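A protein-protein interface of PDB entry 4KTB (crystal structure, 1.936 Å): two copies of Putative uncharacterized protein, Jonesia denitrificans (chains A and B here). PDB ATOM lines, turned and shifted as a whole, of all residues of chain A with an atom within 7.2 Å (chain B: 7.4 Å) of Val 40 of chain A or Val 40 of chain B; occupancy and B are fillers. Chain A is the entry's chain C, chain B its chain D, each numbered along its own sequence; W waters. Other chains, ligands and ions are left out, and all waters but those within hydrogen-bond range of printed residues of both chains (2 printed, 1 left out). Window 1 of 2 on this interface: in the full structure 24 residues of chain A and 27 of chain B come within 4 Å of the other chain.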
ATOM      1  N   LEU A  37       1.190 -15.463 -16.760  1.00  0.00           N
ATOM      2  CA  LEU A  37       0.408 -15.992 -15.641  1.00  0.00           C
ATOM      3  C   LEU A  37       0.131 -17.485 -15.809  1.00  0.00           C
ATOM      4  O   LEU A  37       0.224 -18.012 -16.919  1.00  0.00           O
ATOM      5  CB  LEU A  37      -0.934 -15.261 -15.531  1.00  0.00           C
ATOM      6  CG  LEU A  37      -1.022 -13.739 -15.597  1.00  0.00           C
ATOM      7  CD1 LEU A  37      -2.482 -13.324 -15.605  1.00  0.00           C
ATOM      8  CD2 LEU A  37      -0.306 -13.104 -14.434  1.00  0.00           C
ATOM      9  N   PRO A  38      -0.213 -18.172 -14.703  1.00  0.00           N
ATOM     10  CA  PRO A  38      -0.635 -19.575 -14.800  1.00  0.00           C
ATOM     11  C   PRO A  38      -1.967 -19.739 -15.527  1.00  0.00           C
ATOM     12  O   PRO A  38      -2.832 -18.864 -15.432  1.00  0.00           O
ATOM     13  CB  PRO A  38      -0.774 -20.015 -13.337  1.00  0.00           C
ATOM     14  CG  PRO A  38      -0.836 -18.763 -12.540  1.00  0.00           C
ATOM     15  CD  PRO A  38      -0.046 -17.744 -13.303  1.00  0.00           C
ATOM     16  N   LEU A  39      -2.122 -20.849 -16.247  1.00  0.00           N
ATOM     17  CA  LEU A  39      -3.352 -21.149 -16.971  1.00  0.00           C
ATOM     18  C   LEU A  39      -4.168 -22.167 -16.195  1.00  0.00           C
ATOM     19  O   LEU A  39      -3.613 -23.150 -15.699  1.00  0.00           O
ATOM     20  CB  LEU A  39      -3.039 -21.758 -18.333  1.00  0.00           C
ATOM     21  CG  LEU A  39      -1.974 -21.095 -19.189  1.00  0.00           C
ATOM     22  CD1 LEU A  39      -1.732 -21.922 -20.424  1.00  0.00           C
ATOM     23  CD2 LEU A  39      -2.460 -19.726 -19.566  1.00  0.00           C
ATOM     24  N   VAL A  40      -5.477 -21.939 -16.104  1.00  0.00           N
ATOM     25  CA  VAL A  40      -6.385 -22.925 -15.524  1.00  0.00           C
ATOM     26  C   VAL A  40      -6.630 -24.035 -16.543  1.00  0.00           C
ATOM     27  O   VAL A  40      -7.058 -23.782 -17.670  1.00  0.00           O
ATOM     28  CB  VAL A  40      -7.725 -22.309 -15.090  1.00  0.00           C
ATOM     29  CG1 VAL A  40      -8.609 -23.363 -14.450  1.00  0.00           C
ATOM     30  CG2 VAL A  40      -7.488 -21.178 -14.114  1.00  0.00           C
ATOM     31  N   TYR A  41      -6.346 -25.265 -16.140  1.00  0.00           N
ATOM     32  CA  TYR A  41      -6.496 -26.418 -17.004  1.00  0.00           C
ATOM     33  C   TYR A  41      -7.393 -27.446 -16.329  1.00  0.00           C
ATOM     34  O   TYR A  41      -7.709 -27.330 -15.151  1.00  0.00           O
ATOM     35  CB  TYR A  41      -5.132 -27.051 -17.240  1.00  0.00           C
ATOM     36  CG  TYR A  41      -4.478 -26.714 -18.556  1.00  0.00           C
ATOM     37  CD1 TYR A  41      -4.179 -25.407 -18.901  1.00  0.00           C
ATOM     38  CD2 TYR A  41      -4.120 -27.721 -19.432  1.00  0.00           C
ATOM     39  CE1 TYR A  41      -3.557 -25.117 -20.110  1.00  0.00           C
ATOM     40  CE2 TYR A  41      -3.506 -27.449 -20.630  1.00  0.00           C
ATOM     41  CZ  TYR A  41      -3.228 -26.149 -20.970  1.00  0.00           C
ATOM     42  OH  TYR A  41      -2.612 -25.896 -22.175  1.00  0.00           O
ATOM     43  N   VAL A  42      -7.798 -28.458 -17.080  1.00  0.00           N
ATOM     44  CA  VAL A  42      -8.419 -29.635 -16.487  1.00  0.00           C
ATOM     45  C   VAL A  42      -7.781 -30.885 -17.049  1.00  0.00           C
ATOM     46  O   VAL A  42      -7.433 -30.947 -18.233  1.00  0.00           O
ATOM     47  CB  VAL A  42      -9.967 -29.687 -16.684  1.00  0.00           C
ATOM     48  CG1 VAL A  42     -10.655 -28.696 -15.794  1.00  0.00           C
ATOM     49  CG2 VAL A  42     -10.353 -29.464 -18.140  1.00  0.00           C
ATOM     50  N   GLY A  77      -6.923 -30.112 -20.891  1.00  0.00           N
ATOM     51  CA  GLY A  77      -7.178 -28.872 -21.590  1.00  0.00           C
ATOM     52  C   GLY A  77      -7.444 -27.652 -20.739  1.00  0.00           C
ATOM     53  O   GLY A  77      -7.793 -27.738 -19.566  1.00  0.00           O
ATOM     54  N   ARG A  78      -7.300 -26.498 -21.378  1.00  0.00           N
ATOM     55  CA  ARG A  78      -7.452 -25.199 -20.752  1.00  0.00           C
ATOM     56  C   ARG A  78      -8.911 -24.887 -20.400  1.00  0.00           C
ATOM     57  O   ARG A  78      -9.834 -25.361 -21.065  1.00  0.00           O
ATOM     58  CB  ARG A  78      -6.916 -24.157 -21.731  1.00  0.00           C
ATOM     59  CG  ARG A  78      -6.771 -22.764 -21.191  1.00  0.00           C
ATOM     60  CD  ARG A  78      -6.135 -21.868 -22.255  1.00  0.00           C
ATOM     61  NE  ARG A  78      -7.038 -21.564 -23.368  1.00  0.00           N
ATOM     62  CZ  ARG A  78      -7.853 -20.512 -23.405  1.00  0.00           C
ATOM     63  NH1 ARG A  78      -7.885 -19.665 -22.384  1.00  0.00           N
ATOM     64  NH2 ARG A  78      -8.639 -20.305 -24.455  1.00  0.00           N
ATOM     65  N   VAL A  79      -9.120 -24.112 -19.341  1.00  0.00           N
ATOM     66  CA  VAL A  79     -10.445 -23.589 -19.020  1.00  0.00           C
ATOM     67  C   VAL A  79     -10.546 -22.205 -19.626  1.00  0.00           C
ATOM     68  O   VAL A  79      -9.588 -21.441 -19.573  1.00  0.00           O
ATOM     69  CB  VAL A  79     -10.668 -23.520 -17.506  1.00  0.00           C
ATOM     70  CG1 VAL A  79     -11.985 -22.814 -17.170  1.00  0.00           C
ATOM     71  CG2 VAL A  79     -10.668 -24.921 -16.939  1.00  0.00           C
ATOM     72  N   MET A  80     -11.682 -21.879 -20.227  1.00  0.00           N
ATOM     73  CA  MET A  80     -11.814 -20.595 -20.896  1.00  0.00           C
ATOM     74  C   MET A  80     -12.403 -19.530 -19.978  1.00  0.00           C
ATOM     75  O   MET A  80     -13.092 -19.837 -19.007  1.00  0.00           O
ATOM     76  CB  MET A  80     -12.660 -20.729 -22.165  1.00  0.00           C
ATOM     77  CG  MET A  80     -12.220 -21.872 -23.072  1.00  0.00           C
ATOM     78  SD  MET A  80     -12.889 -21.807 -24.912  1.00  0.00           S
ATOM     79  CE  MET A  80     -14.721 -21.290 -24.517  1.00  0.00           C
ATOM     80  N   VAL A  85     -15.711 -24.869 -14.929  1.00  0.00           N
ATOM     81  CA  VAL A  85     -14.827 -26.017 -14.973  1.00  0.00           C
ATOM     82  C   VAL A  85     -15.506 -27.300 -15.454  1.00  0.00           C
ATOM     83  O   VAL A  85     -14.985 -27.978 -16.339  1.00  0.00           O
ATOM     84  CB  VAL A  85     -14.210 -26.243 -13.598  1.00  0.00           C
ATOM     85  CG1 VAL A  85     -13.298 -27.449 -13.618  1.00  0.00           C
ATOM     86  CG2 VAL A  85     -13.445 -25.001 -13.177  1.00  0.00           C
ATOM     87  N   HIS A  92     -14.120 -30.771 -23.173  1.00  0.00           N
ATOM     88  CA  HIS A  92     -12.890 -31.475 -23.516  1.00  0.00           C
ATOM     89  C   HIS A  92     -13.112 -32.963 -23.770  1.00  0.00           C
ATOM     90  O   HIS A  92     -12.496 -33.543 -24.660  1.00  0.00           O
ATOM     91  CB  HIS A  92     -11.797 -31.247 -22.471  1.00  0.00           C
ATOM     92  CG  HIS A  92     -11.140 -29.907 -22.573  1.00  0.00           C
ATOM     93  ND1 HIS A  92     -10.403 -29.519 -23.671  1.00  0.00           N
ATOM     94  CD2 HIS A  92     -11.111 -28.860 -21.710  1.00  0.00           C
ATOM     95  CE1 HIS A  92      -9.953 -28.290 -23.484  1.00  0.00           C
ATOM     96  NE2 HIS A  92     -10.365 -27.872 -22.300  1.00  0.00           N
ATOM     97  N   HIS A 132       2.929 -22.310 -17.609  1.00  0.00           N
ATOM     98  CA  HIS A 132       2.713 -22.740 -16.243  1.00  0.00           C
ATOM     99  C   HIS A 132       1.223 -22.971 -16.154  1.00  0.00           C
ATOM    100  O   HIS A 132       0.436 -22.035 -16.300  1.00  0.00           O
ATOM    101  CB  HIS A 132       3.146 -21.670 -15.243  1.00  0.00           C
ATOM    102  CG  HIS A 132       2.736 -21.953 -13.825  1.00  0.00           C
ATOM    103  ND1 HIS A 132       2.700 -20.975 -12.861  1.00  0.00           N
ATOM    104  CD2 HIS A 132       2.347 -23.100 -13.218  1.00  0.00           C
ATOM    105  CE1 HIS A 132       2.302 -21.505 -11.713  1.00  0.00           C
ATOM    106  NE2 HIS A 132       2.081 -22.789 -11.906  1.00  0.00           N
ATOM    107  N   ALA A 133       0.847 -24.226 -15.948  1.00  0.00           N
ATOM    108  CA  ALA A 133      -0.551 -24.607 -15.912  1.00  0.00           C
ATOM    109  C   ALA A 133      -0.876 -25.251 -14.564  1.00  0.00           C
ATOM    110  O   ALA A 133      -0.126 -26.092 -14.066  1.00  0.00           O
ATOM    111  CB  ALA A 133      -0.879 -25.551 -17.052  1.00  0.00           C
ATOM    112  N   VAL A 134      -1.998 -24.828 -13.987  1.00  0.00           N
ATOM    113  CA  VAL A 134      -2.504 -25.393 -12.744  1.00  0.00           C
ATOM    114  C   VAL A 134      -3.807 -26.118 -13.071  1.00  0.00           C
ATOM    115  O   VAL A 134      -4.803 -25.480 -13.430  1.00  0.00           O
ATOM    116  CB  VAL A 134      -2.765 -24.302 -11.685  1.00  0.00           C
ATOM    117  CG1 VAL A 134      -3.434 -24.903 -10.457  1.00  0.00           C
ATOM    118  CG2 VAL A 134      -1.475 -23.606 -11.281  1.00  0.00           C
ATOM    119  N   SER A 135      -3.806 -27.443 -12.964  1.00  0.00           N
ATOM    120  CA  SER A 135      -4.934 -28.233 -13.471  1.00  0.00           C
ATOM    121  C   SER A 135      -5.746 -28.906 -12.372  1.00  0.00           C
ATOM    122  O   SER A 135      -5.191 -29.480 -11.432  1.00  0.00           O
ATOM    123  CB  SER A 135      -4.455 -29.280 -14.483  1.00  0.00           C
ATOM    124  OG  SER A 135      -5.531 -29.762 -15.259  1.00  0.00           O
ATOM    125  N   LEU A 136      -7.066 -28.823 -12.484  1.00  0.00           N
ATOM    126  CA  LEU A 136      -7.930 -29.563 -11.582  1.00  0.00           C
ATOM    127  C   LEU A 136      -8.120 -30.907 -12.232  1.00  0.00           C
ATOM    128  O   LEU A 136      -8.594 -30.986 -13.363  1.00  0.00           O
ATOM    129  CB  LEU A 136      -9.283 -28.875 -11.439  1.00  0.00           C
ATOM    130  CG  LEU A 136      -9.261 -27.489 -10.814  1.00  0.00           C
ATOM    131  CD1 LEU A 136     -10.661 -26.886 -10.853  1.00  0.00           C
ATOM    132  CD2 LEU A 136      -8.746 -27.538  -9.390  1.00  0.00           C
ATOM    133  N   LEU B  37      -8.487 -13.744 -19.857  1.00  0.00           N
ATOM    134  CA  LEU B  37      -8.087 -14.953 -19.148  1.00  0.00           C
ATOM    135  C   LEU B  37      -8.815 -15.125 -17.826  1.00  0.00           C
ATOM    136  O   LEU B  37      -9.189 -14.143 -17.175  1.00  0.00           O
ATOM    137  CB  LEU B  37      -6.581 -14.940 -18.874  1.00  0.00           C
ATOM    138  CG  LEU B  37      -5.675 -14.773 -20.088  1.00  0.00           C
ATOM    139  CD1 LEU B  37      -4.203 -14.830 -19.697  1.00  0.00           C
ATOM    140  CD2 LEU B  37      -6.002 -15.849 -21.082  1.00  0.00           C
ATOM    141  N   PRO B  38      -9.029 -16.390 -17.434  1.00  0.00           N
ATOM    142  CA  PRO B  38      -9.407 -16.720 -16.059  1.00  0.00           C
ATOM    143  C   PRO B  38      -8.143 -16.825 -15.207  1.00  0.00           C
ATOM    144  O   PRO B  38      -7.131 -17.347 -15.688  1.00  0.00           O
ATOM    145  CB  PRO B  38     -10.064 -18.094 -16.197  1.00  0.00           C
ATOM    146  CG  PRO B  38      -9.419 -18.701 -17.398  1.00  0.00           C
ATOM    147  CD  PRO B  38      -9.078 -17.565 -18.326  1.00  0.00           C
ATOM    148  N   LEU B  39      -8.204 -16.339 -13.968  1.00  0.00           N
ATOM    149  CA  LEU B  39      -7.033 -16.274 -13.088  1.00  0.00           C
ATOM    150  C   LEU B  39      -7.012 -17.404 -12.067  1.00  0.00           C
ATOM    151  O   LEU B  39      -8.034 -17.686 -11.445  1.00  0.00           O
ATOM    152  CB  LEU B  39      -7.037 -14.955 -12.322  1.00  0.00           C
ATOM    153  CG  LEU B  39      -7.235 -13.728 -13.200  1.00  0.00           C
ATOM    154  CD1 LEU B  39      -7.249 -12.462 -12.374  1.00  0.00           C
ATOM    155  CD2 LEU B  39      -6.112 -13.699 -14.210  1.00  0.00           C
ATOM    156  N   VAL B  40      -5.845 -18.029 -11.890  1.00  0.00           N
ATOM    157  CA  VAL B  40      -5.650 -19.030 -10.837  1.00  0.00           C
ATOM    158  C   VAL B  40      -5.574 -18.335  -9.485  1.00  0.00           C
ATOM    159  O   VAL B  40      -4.755 -17.441  -9.286  1.00  0.00           O
ATOM    160  CB  VAL B  40      -4.369 -19.850 -11.048  1.00  0.00           C
ATOM    161  CG1 VAL B  40      -4.289 -20.978 -10.037  1.00  0.00           C
ATOM    162  CG2 VAL B  40      -4.333 -20.405 -12.459  1.00  0.00           C
ATOM    163  N   TYR B  41      -6.419 -18.761  -8.554  1.00  0.00           N
ATOM    164  CA  TYR B  41      -6.575 -18.072  -7.287  1.00  0.00           C
ATOM    165  C   TYR B  41      -6.545 -19.069  -6.143  1.00  0.00           C
ATOM    166  O   TYR B  41      -6.708 -20.267  -6.345  1.00  0.00           O
ATOM    167  CB  TYR B  41      -7.910 -17.329  -7.274  1.00  0.00           C
ATOM    168  CG  TYR B  41      -7.805 -15.844  -7.041  1.00  0.00           C
ATOM    169  CD1 TYR B  41      -7.183 -15.016  -7.962  1.00  0.00           C
ATOM    170  CD2 TYR B  41      -8.355 -15.267  -5.911  1.00  0.00           C
ATOM    171  CE1 TYR B  41      -7.097 -13.646  -7.744  1.00  0.00           C
ATOM    172  CE2 TYR B  41      -8.278 -13.909  -5.683  1.00  0.00           C
ATOM    173  CZ  TYR B  41      -7.645 -13.099  -6.599  1.00  0.00           C
ATOM    174  OH  TYR B  41      -7.566 -11.738  -6.377  1.00  0.00           O
ATOM    175  N   VAL B  42      -6.325 -18.574  -4.935  1.00  0.00           N
ATOM    176  CA  VAL B  42      -6.550 -19.389  -3.756  1.00  0.00           C
ATOM    177  C   VAL B  42      -7.401 -18.614  -2.785  1.00  0.00           C
ATOM    178  O   VAL B  42      -7.421 -17.376  -2.797  1.00  0.00           O
ATOM    179  CB  VAL B  42      -5.236 -19.835  -3.055  1.00  0.00           C
ATOM    180  CG1 VAL B  42      -4.524 -20.906  -3.861  1.00  0.00           C
ATOM    181  CG2 VAL B  42      -4.327 -18.638  -2.794  1.00  0.00           C
ATOM    182  N   GLY B  77      -6.307 -14.341  -2.976  1.00  0.00           N
ATOM    183  CA  GLY B  77      -5.429 -13.590  -3.836  1.00  0.00           C
ATOM    184  C   GLY B  77      -4.882 -14.503  -4.898  1.00  0.00           C
ATOM    185  O   GLY B  77      -5.090 -15.710  -4.869  1.00  0.00           O
ATOM    186  N   ARG B  78      -4.153 -13.913  -5.828  1.00  0.00           N
ATOM    187  CA  ARG B  78      -3.671 -14.598  -7.009  1.00  0.00           C
ATOM    188  C   ARG B  78      -2.496 -15.523  -6.712  1.00  0.00           C
ATOM    189  O   ARG B  78      -1.745 -15.299  -5.762  1.00  0.00           O
ATOM    190  CB  ARG B  78      -3.231 -13.537  -8.012  1.00  0.00           C
ATOM    191  CG  ARG B  78      -3.038 -14.044  -9.409  1.00  0.00           C
ATOM    192  CD  ARG B  78      -2.863 -12.895 -10.391  1.00  0.00           C
ATOM    193  NE  ARG B  78      -1.542 -12.276 -10.306  1.00  0.00           N
ATOM    194  CZ  ARG B  78      -0.426 -12.831 -10.771  1.00  0.00           C
ATOM    195  NH1 ARG B  78      -0.467 -14.031 -11.334  1.00  0.00           N
ATOM    196  NH2 ARG B  78       0.732 -12.190 -10.663  1.00  0.00           N
ATOM    197  N   VAL B  79      -2.340 -16.563  -7.525  1.00  0.00           N
ATOM    198  CA  VAL B  79      -1.125 -17.364  -7.519  1.00  0.00           C
ATOM    199  C   VAL B  79      -0.246 -16.875  -8.642  1.00  0.00           C
ATOM    200  O   VAL B  79      -0.588 -17.019  -9.807  1.00  0.00           O
ATOM    201  CB  VAL B  79      -1.409 -18.843  -7.768  1.00  0.00           C
ATOM    202  CG1 VAL B  79      -0.096 -19.601  -7.947  1.00  0.00           C
ATOM    203  CG2 VAL B  79      -2.215 -19.423  -6.626  1.00  0.00           C
ATOM    204  N   MET B  80       0.886 -16.294  -8.296  1.00  0.00           N
ATOM    205  CA  MET B  80       1.744 -15.702  -9.302  1.00  0.00           C
ATOM    206  C   MET B  80       2.409 -16.739 -10.199  1.00  0.00           C
ATOM    207  O   MET B  80       2.559 -17.894  -9.825  1.00  0.00           O
ATOM    208  CB  MET B  80       2.796 -14.831  -8.633  1.00  0.00           C
ATOM    209  CG  MET B  80       2.292 -13.439  -8.255  1.00  0.00           C
ATOM    210  SD  MET B  80       3.264 -12.742  -6.735  1.00  0.00           S
ATOM    211  CE  MET B  80       4.977 -13.616  -7.085  1.00  0.00           C
ATOM    212  N   GLU B  83       4.724 -19.739  -9.312  1.00  0.00           N
ATOM    213  CA  GLU B  83       4.545 -19.932  -7.873  1.00  0.00           C
ATOM    214  C   GLU B  83       3.646 -21.138  -7.604  1.00  0.00           C
ATOM    215  O   GLU B  83       2.592 -21.289  -8.225  1.00  0.00           O
ATOM    216  CB  GLU B  83       3.945 -18.679  -7.235  1.00  0.00           C
ATOM    217  CG  GLU B  83       3.455 -18.858  -5.823  1.00  0.00           C
ATOM    218  CD  GLU B  83       2.927 -17.570  -5.233  1.00  0.00           C
ATOM    219  OE1 GLU B  83       2.122 -16.882  -5.901  1.00  0.00           O
ATOM    220  OE2 GLU B  83       3.320 -17.240  -4.096  1.00  0.00           O
ATOM    221  N   VAL B  85       0.964 -23.496  -5.640  1.00  0.00           N
ATOM    222  CA  VAL B  85      -0.231 -23.228  -4.857  1.00  0.00           C
ATOM    223  C   VAL B  85       0.059 -23.134  -3.353  1.00  0.00           C
ATOM    224  O   VAL B  85      -0.316 -22.153  -2.712  1.00  0.00           O
ATOM    225  CB  VAL B  85      -1.328 -24.278  -5.132  1.00  0.00           C
ATOM    226  CG1 VAL B  85      -2.558 -24.005  -4.287  1.00  0.00           C
ATOM    227  CG2 VAL B  85      -1.706 -24.271  -6.598  1.00  0.00           C
ATOM    228  N   ALA B  88       1.723 -19.944  -2.534  1.00  0.00           N
ATOM    229  CA  ALA B  88       0.893 -18.755  -2.642  1.00  0.00           C
ATOM    230  C   ALA B  88       0.017 -18.705  -1.413  1.00  0.00           C
ATOM    231  O   ALA B  88      -0.371 -17.634  -0.943  1.00  0.00           O
ATOM    232  CB  ALA B  88       0.056 -18.808  -3.887  1.00  0.00           C
ATOM    233  N   VAL B 114     -13.669 -25.980  -5.163  1.00  0.00           N
ATOM    234  CA  VAL B 114     -13.180 -25.046  -6.152  1.00  0.00           C
ATOM    235  C   VAL B 114     -14.216 -23.945  -6.386  1.00  0.00           C
ATOM    236  O   VAL B 114     -15.301 -24.195  -6.909  1.00  0.00           O
ATOM    237  CB  VAL B 114     -12.853 -25.762  -7.459  1.00  0.00           C
ATOM    238  CG1 VAL B 114     -12.511 -24.750  -8.542  1.00  0.00           C
ATOM    239  CG2 VAL B 114     -11.709 -26.756  -7.250  1.00  0.00           C
ATOM    240  N   HIS B 132     -12.608 -13.087 -13.797  1.00  0.00           N
ATOM    241  CA  HIS B 132     -12.950 -14.482 -13.612  1.00  0.00           C
ATOM    242  C   HIS B 132     -11.798 -15.135 -12.874  1.00  0.00           C
ATOM    243  O   HIS B 132     -10.680 -15.183 -13.396  1.00  0.00           O
ATOM    244  CB  HIS B 132     -13.132 -15.169 -14.964  1.00  0.00           C
ATOM    245  CG  HIS B 132     -13.459 -16.632 -14.867  1.00  0.00           C
ATOM    246  ND1 HIS B 132     -13.349 -17.486 -15.939  1.00  0.00           N
ATOM    247  CD2 HIS B 132     -13.903 -17.384 -13.830  1.00  0.00           C
ATOM    248  CE1 HIS B 132     -13.706 -18.707 -15.569  1.00  0.00           C
ATOM    249  NE2 HIS B 132     -14.044 -18.670 -14.295  1.00  0.00           N
ATOM    250  N   ALA B 133     -12.071 -15.637 -11.671  1.00  0.00           N
ATOM    251  CA  ALA B 133     -11.042 -16.245 -10.840  1.00  0.00           C
ATOM    252  C   ALA B 133     -11.435 -17.668 -10.457  1.00  0.00           C
ATOM    253  O   ALA B 133     -12.473 -17.885  -9.831  1.00  0.00           O
ATOM    254  CB  ALA B 133     -10.795 -15.408  -9.597  1.00  0.00           C
ATOM    255  N   VAL B 134     -10.590 -18.626 -10.831  1.00  0.00           N
ATOM    256  CA  VAL B 134     -10.783 -20.026 -10.473  1.00  0.00           C
ATOM    257  C   VAL B 134     -10.045 -20.285  -9.158  1.00  0.00           C
ATOM    258  O   VAL B 134      -8.829 -20.486  -9.152  1.00  0.00           O
ATOM    259  CB  VAL B 134     -10.252 -20.968 -11.576  1.00  0.00           C
ATOM    260  CG1 VAL B 134     -10.281 -22.415 -11.108  1.00  0.00           C
ATOM    261  CG2 VAL B 134     -11.062 -20.813 -12.863  1.00  0.00           C
ATOM    262  N   SER B 135     -10.779 -20.276  -8.048  1.00  0.00           N
ATOM    263  CA  SER B 135     -10.158 -20.207  -6.721  1.00  0.00           C
ATOM    264  C   SER B 135     -10.109 -21.553  -5.998  1.00  0.00           C
ATOM    265  O   SER B 135     -11.143 -22.168  -5.754  1.00  0.00           O
ATOM    266  CB  SER B 135     -10.894 -19.185  -5.853  1.00  0.00           C
ATOM    267  OG  SER B 135     -10.416 -19.224  -4.524  1.00  0.00           O
ATOM    268  N   LEU B 136      -8.908 -22.000  -5.648  1.00  0.00           N
ATOM    269  CA  LEU B 136      -8.749 -23.260  -4.932  1.00  0.00           C
ATOM    270  C   LEU B 136      -8.862 -23.009  -3.430  1.00  0.00           C
ATOM    271  O   LEU B 136      -8.043 -22.297  -2.845  1.00  0.00           O
ATOM    272  CB  LEU B 136      -7.403 -23.909  -5.255  1.00  0.00           C
ATOM    273  CG  LEU B 136      -6.928 -23.851  -6.704  1.00  0.00           C
ATOM    274  CD1 LEU B 136      -5.640 -24.663  -6.899  1.00  0.00           C
ATOM    275  CD2 LEU B 136      -7.987 -24.327  -7.650  1.00  0.00           C
HETATM  276  O   HOH W   1      -5.821 -19.141 -17.356  1.00  0.00           O
HETATM  277  O   HOH W   2       1.332 -23.991  -9.471  1.00  0.00           O
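Of chain B, only Val 40 and Val 134 come within 4 Å of Val 40 of chain A.
Val 42 of chain A touches none of the printed residues of chain B.
Printed residues of chain B within 4 Å of Val 79 of chain A: Pro 38.
Of the printed residues of chain B, His 132 of chain A touches Glu 83.
Printed residues of chain A within 4 Å of Leu 39 of chain B: Leu 37.
Of the printed residues of chain A, Val 40 of chain B touches Pro 38 (3.7 Å) and Val 40 (3.6 Å).
Val 42 of chain B touches none of the printed residues of chain A.
The nearest printed residue of chain A that does not touch Val 40 of chain B is Val 134 of chain A (4.01 Å).
Water W1 lies within hydrogen-bond range of O of Pro 38 of chain B (2.8 Å) and N of Val 40 of chain A (3.1 Å).
Water W2 lies within hydrogen-bond range of a ring nitrogen (NE2) of His 132 of chain A (2.8 Å) and the backbone carbonyl oxygen of Glu 83 of chain B (3.2 Å).
Leu 37 of chain A touches Arg 78 of chain B, but with the chains exchanged Arg 78 of chain A does not touch Leu 37 of chain B (4.5 Å).
Val 40 of chain B touches its own counterpart, Val 40 of chain A.
Val 40 of chain A touches Val 134 of chain B, but with the chains exchanged Val 134 of chain A does not touch Val 40 of chain B (4.01 Å).
Leu 136 of chain A touches its own counterpart, Leu 136 of chain B.
Positions printed for both chains: 37, 38, 39, 40, 41, 42, 77, 78, 79, 80, 85, 132, 133, 134, 135 and 136.
O of Val 134 of chain B lies within hydrogen-bond range of N of Tyr 41 of chain B (3.0 Å).
The backbone carbonyl oxygen (O) of Tyr 41 of chain B sits at hydrogen-bond distance from the backbone NH (N) of Leu 136 of chain B (2.9 Å).
The backbone carbonyl oxygen of Tyr 41 of chain A sits at hydrogen-bond distance from the backbone NH of Leu 136 of chain A.
The backbone carbonyl oxygen (O) of Leu 39 of chain B lies within hydrogen-bond range of the backbone NH (N) of Val 134 of chain B (2.8 Å).
O of His 132 of chain A lies within hydrogen-bond range of N of Leu 39 of chain A (2.8 Å).
The backbone NH of Met 80 of chain B lies within hydrogen-bond range of the side-chain carboxylate of Glu 83 of chain B (2.8 Å).
Of the 17 printed residues of chain A, 7 touch a printed residue of chain B.
Hydrophobic or aromatic side chains of chain A within 4 Å of the printed part of chain B: Leu 37, Pro 38, Val 40, His 132 and Leu 136.
Hydrophobic or aromatic side chains of chain B within 4 Å of the printed part of chain A: Pro 38, Leu 39, Val 40, Val 114, His 132, Val 134 and Leu 136.
Among the printed residues, pairs that only touch across the chains: Leu 37 of chain A with Leu 39 of chain B, Leu 37 of chain A with Arg 78 of chain B, Pro 38 of chain A with Val 40 of chain B, Pro 38 of chain A with Val 79 of chain B, Val 40 of chain A with Val 40 of chain B, Val 40 of chain A with Val 134 of chain B, Val 79 of chain A with Pro 38 of chain B, Met 80 of chain A with His 132 of chain B, His 132 of chain A with Glu 83 of chain B, Leu 136 of chain A with Val 114 of chain B and Leu 136 of chain A with Leu 136 of chain B.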
